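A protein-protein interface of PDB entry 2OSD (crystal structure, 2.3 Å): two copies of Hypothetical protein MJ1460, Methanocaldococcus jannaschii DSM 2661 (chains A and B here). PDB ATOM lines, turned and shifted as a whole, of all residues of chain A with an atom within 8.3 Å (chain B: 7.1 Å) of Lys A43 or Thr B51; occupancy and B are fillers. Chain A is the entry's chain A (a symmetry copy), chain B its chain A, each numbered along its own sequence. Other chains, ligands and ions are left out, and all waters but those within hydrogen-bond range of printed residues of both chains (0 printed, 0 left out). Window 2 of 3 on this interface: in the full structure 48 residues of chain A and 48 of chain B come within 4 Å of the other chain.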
ATOM      1  N   GLU A   6      23.855  -5.947  -7.079  1.00  0.00           N
ATOM      2  CA  GLU A   6      22.946  -6.000  -5.894  1.00  0.00           C
ATOM      3  C   GLU A   6      22.387  -4.605  -5.568  1.00  0.00           C
ATOM      4  O   GLU A   6      22.945  -3.587  -5.998  1.00  0.00           O
ATOM      5  CB  GLU A   6      23.679  -6.600  -4.688  1.00  0.00           C
ATOM      6  N   PHE A  36      34.230 -15.326   2.818  1.00  0.00           N
ATOM      7  CA  PHE A  36      33.455 -14.767   1.706  1.00  0.00           C
ATOM      8  C   PHE A  36      34.227 -14.892   0.420  1.00  0.00           C
ATOM      9  O   PHE A  36      33.678 -15.352  -0.599  1.00  0.00           O
ATOM     10  CB  PHE A  36      33.096 -13.308   1.923  1.00  0.00           C
ATOM     11  CG  PHE A  36      32.153 -12.746   0.871  1.00  0.00           C
ATOM     12  CD1 PHE A  36      32.594 -12.503  -0.450  1.00  0.00           C
ATOM     13  CD2 PHE A  36      30.832 -12.456   1.198  1.00  0.00           C
ATOM     14  CE1 PHE A  36      31.707 -11.997  -1.444  1.00  0.00           C
ATOM     15  CE2 PHE A  36      29.961 -11.925   0.255  1.00  0.00           C
ATOM     16  CZ  PHE A  36      30.395 -11.692  -1.076  1.00  0.00           C
ATOM     17  N   ALA A  37      35.499 -14.517   0.451  1.00  0.00           N
ATOM     18  CA  ALA A  37      36.316 -14.576  -0.751  1.00  0.00           C
ATOM     19  C   ALA A  37      36.435 -15.988  -1.208  1.00  0.00           C
ATOM     20  O   ALA A  37      36.324 -16.246  -2.405  1.00  0.00           O
ATOM     21  CB  ALA A  37      37.676 -14.020  -0.503  1.00  0.00           C
ATOM     22  N   LEU A  38      36.683 -16.912  -0.276  1.00  0.00           N
ATOM     23  CA  LEU A  38      36.859 -18.315  -0.628  1.00  0.00           C
ATOM     24  C   LEU A  38      35.624 -18.887  -1.338  1.00  0.00           C
ATOM     25  O   LEU A  38      35.756 -19.639  -2.314  1.00  0.00           O
ATOM     26  CB  LEU A  38      37.169 -19.140   0.630  1.00  0.00           C
ATOM     27  CG  LEU A  38      37.396 -20.659   0.583  1.00  0.00           C
ATOM     28  CD1 LEU A  38      37.932 -21.075   1.951  1.00  0.00           C
ATOM     29  CD2 LEU A  38      36.174 -21.561   0.174  1.00  0.00           C
ATOM     30  N   VAL A  39      34.435 -18.534  -0.838  1.00  0.00           N
ATOM     31  CA  VAL A  39      33.168 -19.048  -1.374  1.00  0.00           C
ATOM     32  C   VAL A  39      32.914 -18.498  -2.801  1.00  0.00           C
ATOM     33  O   VAL A  39      32.489 -19.233  -3.682  1.00  0.00           O
ATOM     34  CB  VAL A  39      31.973 -18.714  -0.426  1.00  0.00           C
ATOM     35  CG1 VAL A  39      30.658 -18.976  -1.120  1.00  0.00           C
ATOM     36  CG2 VAL A  39      32.068 -19.517   0.886  1.00  0.00           C
ATOM     37  N   ILE A  40      33.187 -17.217  -3.020  1.00  0.00           N
ATOM     38  CA  ILE A  40      33.039 -16.625  -4.351  1.00  0.00           C
ATOM     39  C   ILE A  40      33.978 -17.270  -5.349  1.00  0.00           C
ATOM     40  O   ILE A  40      33.542 -17.760  -6.383  1.00  0.00           O
ATOM     41  CB  ILE A  40      33.321 -15.143  -4.381  1.00  0.00           C
ATOM     42  CG1 ILE A  40      32.354 -14.395  -3.481  1.00  0.00           C
ATOM     43  CG2 ILE A  40      33.106 -14.613  -5.793  1.00  0.00           C
ATOM     44  CD1 ILE A  40      31.792 -13.154  -4.172  1.00  0.00           C
ATOM     45  N   PHE A  41      35.263 -17.303  -5.030  1.00  0.00           N
ATOM     46  CA  PHE A  41      36.227 -17.982  -5.881  1.00  0.00           C
ATOM     47  C   PHE A  41      35.842 -19.421  -6.238  1.00  0.00           C
ATOM     48  O   PHE A  41      36.393 -19.991  -7.166  1.00  0.00           O
ATOM     49  CB  PHE A  41      37.604 -17.958  -5.226  1.00  0.00           C
ATOM     50  CG  PHE A  41      38.396 -16.748  -5.571  1.00  0.00           C
ATOM     51  CD1 PHE A  41      37.976 -15.498  -5.168  1.00  0.00           C
ATOM     52  CD2 PHE A  41      39.551 -16.853  -6.337  1.00  0.00           C
ATOM     53  CE1 PHE A  41      38.696 -14.375  -5.507  1.00  0.00           C
ATOM     54  CE2 PHE A  41      40.279 -15.732  -6.673  1.00  0.00           C
ATOM     55  CZ  PHE A  41      39.851 -14.494  -6.257  1.00  0.00           C
ATOM     56  N   ASP A  42      34.912 -20.010  -5.498  1.00  0.00           N
ATOM     57  CA  ASP A  42      34.406 -21.351  -5.795  1.00  0.00           C
ATOM     58  C   ASP A  42      33.264 -21.307  -6.817  1.00  0.00           C
ATOM     59  O   ASP A  42      32.950 -22.317  -7.465  1.00  0.00           O
ATOM     60  CB  ASP A  42      33.911 -22.014  -4.522  1.00  0.00           C
ATOM     61  CG  ASP A  42      34.604 -23.298  -4.263  1.00  0.00           C
ATOM     62  OD1 ASP A  42      35.842 -23.238  -4.127  1.00  0.00           O
ATOM     63  OD2 ASP A  42      33.931 -24.354  -4.206  1.00  0.00           O
ATOM     64  N   LYS A  43      32.641 -20.131  -6.925  1.00  0.00           N
ATOM     65  CA  LYS A  43      31.673 -19.816  -7.964  1.00  0.00           C
ATOM     66  C   LYS A  43      32.229 -18.793  -9.007  1.00  0.00           C
ATOM     67  O   LYS A  43      31.517 -18.401  -9.913  1.00  0.00           O
ATOM     68  CB  LYS A  43      30.364 -19.345  -7.294  1.00  0.00           C
ATOM     69  CG  LYS A  43      29.805 -20.362  -6.252  1.00  0.00           C
ATOM     70  CD  LYS A  43      28.419 -19.991  -5.732  1.00  0.00           C
ATOM     71  N   VAL A  44      33.489 -18.362  -8.875  1.00  0.00           N
ATOM     72  CA  VAL A  44      34.229 -17.740  -9.992  1.00  0.00           C
ATOM     73  C   VAL A  44      34.819 -18.878 -10.830  1.00  0.00           C
ATOM     74  O   VAL A  44      35.067 -18.694 -12.007  1.00  0.00           O
ATOM     75  CB  VAL A  44      35.373 -16.713  -9.535  1.00  0.00           C
ATOM     76  CG1 VAL A  44      36.266 -16.252 -10.695  1.00  0.00           C
ATOM     77  CG2 VAL A  44      34.796 -15.476  -8.856  1.00  0.00           C
ATOM     78  N   LYS A  45      35.028 -20.056 -10.238  1.00  0.00           N
ATOM     79  CA  LYS A  45      35.561 -21.225 -10.973  1.00  0.00           C
ATOM     80  C   LYS A  45      34.715 -22.472 -10.741  1.00  0.00           C
ATOM     81  O   LYS A  45      33.772 -22.726 -11.484  1.00  0.00           O
ATOM     82  CB  LYS A  45      37.007 -21.504 -10.560  1.00  0.00           C
ATOM     83  N   GLY A  48      32.555 -19.906 -13.719  1.00  0.00           N
ATOM     84  CA  GLY A  48      33.727 -20.476 -14.381  1.00  0.00           C
ATOM     85  C   GLY A  48      34.564 -19.434 -15.109  1.00  0.00           C
ATOM     86  O   GLY A  48      34.395 -19.227 -16.316  1.00  0.00           O
ATOM     87  N   SER A  49      35.481 -18.798 -14.374  1.00  0.00           N
ATOM     88  CA  SER A  49      36.319 -17.684 -14.875  1.00  0.00           C
ATOM     89  C   SER A  49      37.468 -17.383 -13.872  1.00  0.00           C
ATOM     90  O   SER A  49      37.463 -17.923 -12.753  1.00  0.00           O
ATOM     91  CB  SER A  49      35.454 -16.438 -15.121  1.00  0.00           C
ATOM     92  N   PHE B  41      32.170  -8.808  -7.800  1.00  0.00           N
ATOM     93  CA  PHE B  41      31.082  -8.766  -8.765  1.00  0.00           C
ATOM     94  C   PHE B  41      31.359  -7.879  -9.983  1.00  0.00           C
ATOM     95  O   PHE B  41      30.676  -7.988 -10.988  1.00  0.00           O
ATOM     96  CB  PHE B  41      29.797  -8.318  -8.076  1.00  0.00           C
ATOM     97  CG  PHE B  41      29.021  -9.445  -7.493  1.00  0.00           C
ATOM     98  CD1 PHE B  41      29.540 -10.190  -6.455  1.00  0.00           C
ATOM     99  CD2 PHE B  41      27.778  -9.791  -8.011  1.00  0.00           C
ATOM    100  CE1 PHE B  41      28.832 -11.247  -5.931  1.00  0.00           C
ATOM    101  CE2 PHE B  41      27.063 -10.844  -7.485  1.00  0.00           C
ATOM    102  CZ  PHE B  41      27.591 -11.572  -6.445  1.00  0.00           C
ATOM    103  N   VAL B  44      33.419 -10.449 -11.648  1.00  0.00           N
ATOM    104  CA  VAL B  44      32.575 -11.599 -12.034  1.00  0.00           C
ATOM    105  C   VAL B  44      31.840 -11.206 -13.319  1.00  0.00           C
ATOM    106  O   VAL B  44      31.460 -12.072 -14.085  1.00  0.00           O
ATOM    107  CB  VAL B  44      31.540 -12.068 -10.903  1.00  0.00           C
ATOM    108  CG1 VAL B  44      30.533 -13.113 -11.405  1.00  0.00           C
ATOM    109  CG2 VAL B  44      32.247 -12.638  -9.678  1.00  0.00           C
ATOM    110  N   SER B  49      30.758 -13.446 -15.930  1.00  0.00           N
ATOM    111  CA  SER B  49      29.914 -14.593 -15.523  1.00  0.00           C
ATOM    112  C   SER B  49      28.908 -14.155 -14.420  1.00  0.00           C
ATOM    113  O   SER B  49      29.026 -13.036 -13.892  1.00  0.00           O
ATOM    114  CB  SER B  49      30.795 -15.757 -15.042  1.00  0.00           C
ATOM    115  N   GLU B  50      28.004 -15.069 -14.042  1.00  0.00           N
ATOM    116  CA  GLU B  50      26.791 -14.741 -13.264  1.00  0.00           C
ATOM    117  C   GLU B  50      26.422 -15.744 -12.141  1.00  0.00           C
ATOM    118  O   GLU B  50      26.111 -16.909 -12.424  1.00  0.00           O
ATOM    119  CB  GLU B  50      25.619 -14.591 -14.251  1.00  0.00           C
ATOM    120  CG  GLU B  50      24.235 -15.000 -13.753  1.00  0.00           C
ATOM    121  CD  GLU B  50      23.168 -14.732 -14.793  1.00  0.00           C
ATOM    122  OE1 GLU B  50      22.988 -13.555 -15.164  1.00  0.00           O
ATOM    123  OE2 GLU B  50      22.513 -15.691 -15.243  1.00  0.00           O
ATOM    124  N   THR B  51      26.490 -15.286 -10.879  1.00  0.00           N
ATOM    125  CA  THR B  51      25.854 -15.962  -9.716  1.00  0.00           C
ATOM    126  C   THR B  51      25.059 -14.833  -9.008  1.00  0.00           C
ATOM    127  O   THR B  51      24.987 -13.732  -9.543  1.00  0.00           O
ATOM    128  CB  THR B  51      26.938 -16.567  -8.724  1.00  0.00           C
ATOM    129  OG1 THR B  51      26.347 -17.486  -7.790  1.00  0.00           O
ATOM    130  CG2 THR B  51      27.675 -15.467  -7.936  1.00  0.00           C
ATOM    131  N   SER B  52      24.502 -15.079  -7.820  1.00  0.00           N
ATOM    132  CA  SER B  52      23.845 -14.034  -7.018  1.00  0.00           C
ATOM    133  C   SER B  52      24.347 -14.080  -5.595  1.00  0.00           C
ATOM    134  O   SER B  52      24.984 -15.045  -5.206  1.00  0.00           O
ATOM    135  CB  SER B  52      22.324 -14.211  -7.007  1.00  0.00           C
ATOM    136  OG  SER B  52      21.870 -15.069  -5.975  1.00  0.00           O
ATOM    137  N   LEU B  53      24.032 -13.045  -4.814  1.00  0.00           N
ATOM    138  CA  LEU B  53      24.414 -12.963  -3.399  1.00  0.00           C
ATOM    139  C   LEU B  53      23.660 -13.950  -2.494  1.00  0.00           C
ATOM    140  O   LEU B  53      24.199 -14.427  -1.493  1.00  0.00           O
ATOM    141  CB  LEU B  53      24.223 -11.539  -2.859  1.00  0.00           C
ATOM    142  CG  LEU B  53      25.400 -10.522  -2.850  1.00  0.00           C
ATOM    143  CD1 LEU B  53      24.892  -9.168  -2.287  1.00  0.00           C
ATOM    144  CD2 LEU B  53      26.630 -10.971  -2.066  1.00  0.00           C
ATOM    145  N   TYR B  54      22.408 -14.231  -2.811  1.00  0.00           N
ATOM    146  CA  TYR B  54      21.664 -15.244  -2.078  1.00  0.00           C
ATOM    147  C   TYR B  54      22.425 -16.561  -2.197  1.00  0.00           C
ATOM    148  O   TYR B  54      22.760 -17.172  -1.175  1.00  0.00           O
ATOM    149  CB  TYR B  54      20.220 -15.383  -2.610  1.00  0.00           C
ATOM    150  CG  TYR B  54      19.396 -16.439  -1.879  1.00  0.00           C
ATOM    151  CD1 TYR B  54      18.820 -16.192  -0.626  1.00  0.00           C
ATOM    152  CD2 TYR B  54      19.208 -17.691  -2.439  1.00  0.00           C
ATOM    153  CE1 TYR B  54      18.056 -17.180   0.025  1.00  0.00           C
ATOM    154  CE2 TYR B  54      18.478 -18.649  -1.806  1.00  0.00           C
ATOM    155  CZ  TYR B  54      17.902 -18.406  -0.583  1.00  0.00           C
ATOM    156  OH  TYR B  54      17.179 -19.431   0.000  1.00  0.00           O
ATOM    157  N   GLU B  55      22.732 -16.950  -3.446  1.00  0.00           N
ATOM    158  CA  GLU B  55      23.479 -18.182  -3.740  1.00  0.00           C
ATOM    159  C   GLU B  55      24.842 -18.275  -3.036  1.00  0.00           C
ATOM    160  O   GLU B  55      25.253 -19.354  -2.607  1.00  0.00           O
ATOM    161  CB  GLU B  55      23.641 -18.363  -5.256  1.00  0.00           C
ATOM    162  CG  GLU B  55      22.286 -18.573  -5.977  1.00  0.00           C
ATOM    163  CD  GLU B  55      22.398 -18.846  -7.479  1.00  0.00           C
ATOM    164  OE1 GLU B  55      23.475 -18.622  -8.064  1.00  0.00           O
ATOM    165  OE2 GLU B  55      21.395 -19.293  -8.076  1.00  0.00           O
ATOM    166  N   ILE B  56      25.523 -17.141  -2.882  1.00  0.00           N
ATOM    167  CA  ILE B  56      26.801 -17.098  -2.176  1.00  0.00           C
ATOM    168  C   ILE B  56      26.596 -17.300  -0.677  1.00  0.00           C
ATOM    169  O   ILE B  56      27.295 -18.086  -0.044  1.00  0.00           O
ATOM    170  CB  ILE B  56      27.566 -15.778  -2.489  1.00  0.00           C
ATOM    171  CG1 ILE B  56      28.214 -15.897  -3.872  1.00  0.00           C
ATOM    172  CG2 ILE B  56      28.609 -15.467  -1.407  1.00  0.00           C
ATOM    173  CD1 ILE B  56      28.490 -14.600  -4.483  1.00  0.00           C
ATOM    174  N   GLU B  59      26.052 -20.969   0.041  1.00  0.00           N
ATOM    175  CA  GLU B  59      27.337 -21.691   0.076  1.00  0.00           C
ATOM    176  C   GLU B  59      28.139 -21.362   1.318  1.00  0.00           C
ATOM    177  O   GLU B  59      28.849 -22.192   1.840  1.00  0.00           O
ATOM    178  CB  GLU B  59      28.185 -21.355  -1.158  1.00  0.00           C
ATOM    179  CG  GLU B  59      29.093 -22.479  -1.599  1.00  0.00           C
ATOM    180  CD  GLU B  59      28.293 -23.724  -2.069  1.00  0.00           C
ATOM    181  OE1 GLU B  59      27.353 -23.575  -2.894  1.00  0.00           O
ATOM    182  OE2 GLU B  59      28.597 -24.845  -1.602  1.00  0.00           O
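N of Ser B49 is in hydrogen-bond range of O of Val B44.
The side-chain carboxylate (OE1) of Glu B55 sits at hydrogen-bond distance from the side-chain hydroxyl (OG1) of Thr B51 (3.1 Å).
The backbone carbonyl oxygen of Val A44 is in hydrogen-bond range of the backbone NH of Ser A49.
Among the printed residues, merely in contact across the chains: Val A39 with Glu B59, Ile A40 with Ile B56, Val A39 with Ile B56, Glu A6 with Leu B53, Lys A43 with Thr B51, Val A44 with Val B44, Ile A40 with Phe B41 and Phe A36 with Leu B53.
Thr B51 touches one residue of chain A.
Printed residues of chain A within 4 Å of Glu B59: Val A39 (3.4 Å).
Of the printed residues of chain B, Ile A40 touches Phe B41 (3.9 Å) and Ile B56 (3.6 Å).
The nearest printed residue of chain B that does not touch Lys A43 is Glu B55 (4.5 Å).
The nearest printed residue of chain A that does not touch Glu B59 is Lys A43 (4.7 Å).
Hydrophobic or aromatic side chains of chain A within 4 Å of the printed part of chain B: Phe A36, Val A39, Ile A40 and Val A44.
Of the 11 printed residues of chain B, 6 touch a printed residue of chain A.
Hydrophobic or aromatic side chains of chain B that line the printed part of chain A: Phe B41, Val B44, Leu B53 and Ile B56.
Along chain B the printed residues that touch a printed residue of chain A span positions 41 to 59.
Among the printed residues, no Asp or Glu carboxylate lies within 4 Å of a Lys or Arg side-chain nitrogen of the other chain.
Val A44 touches its own counterpart, Val B44.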
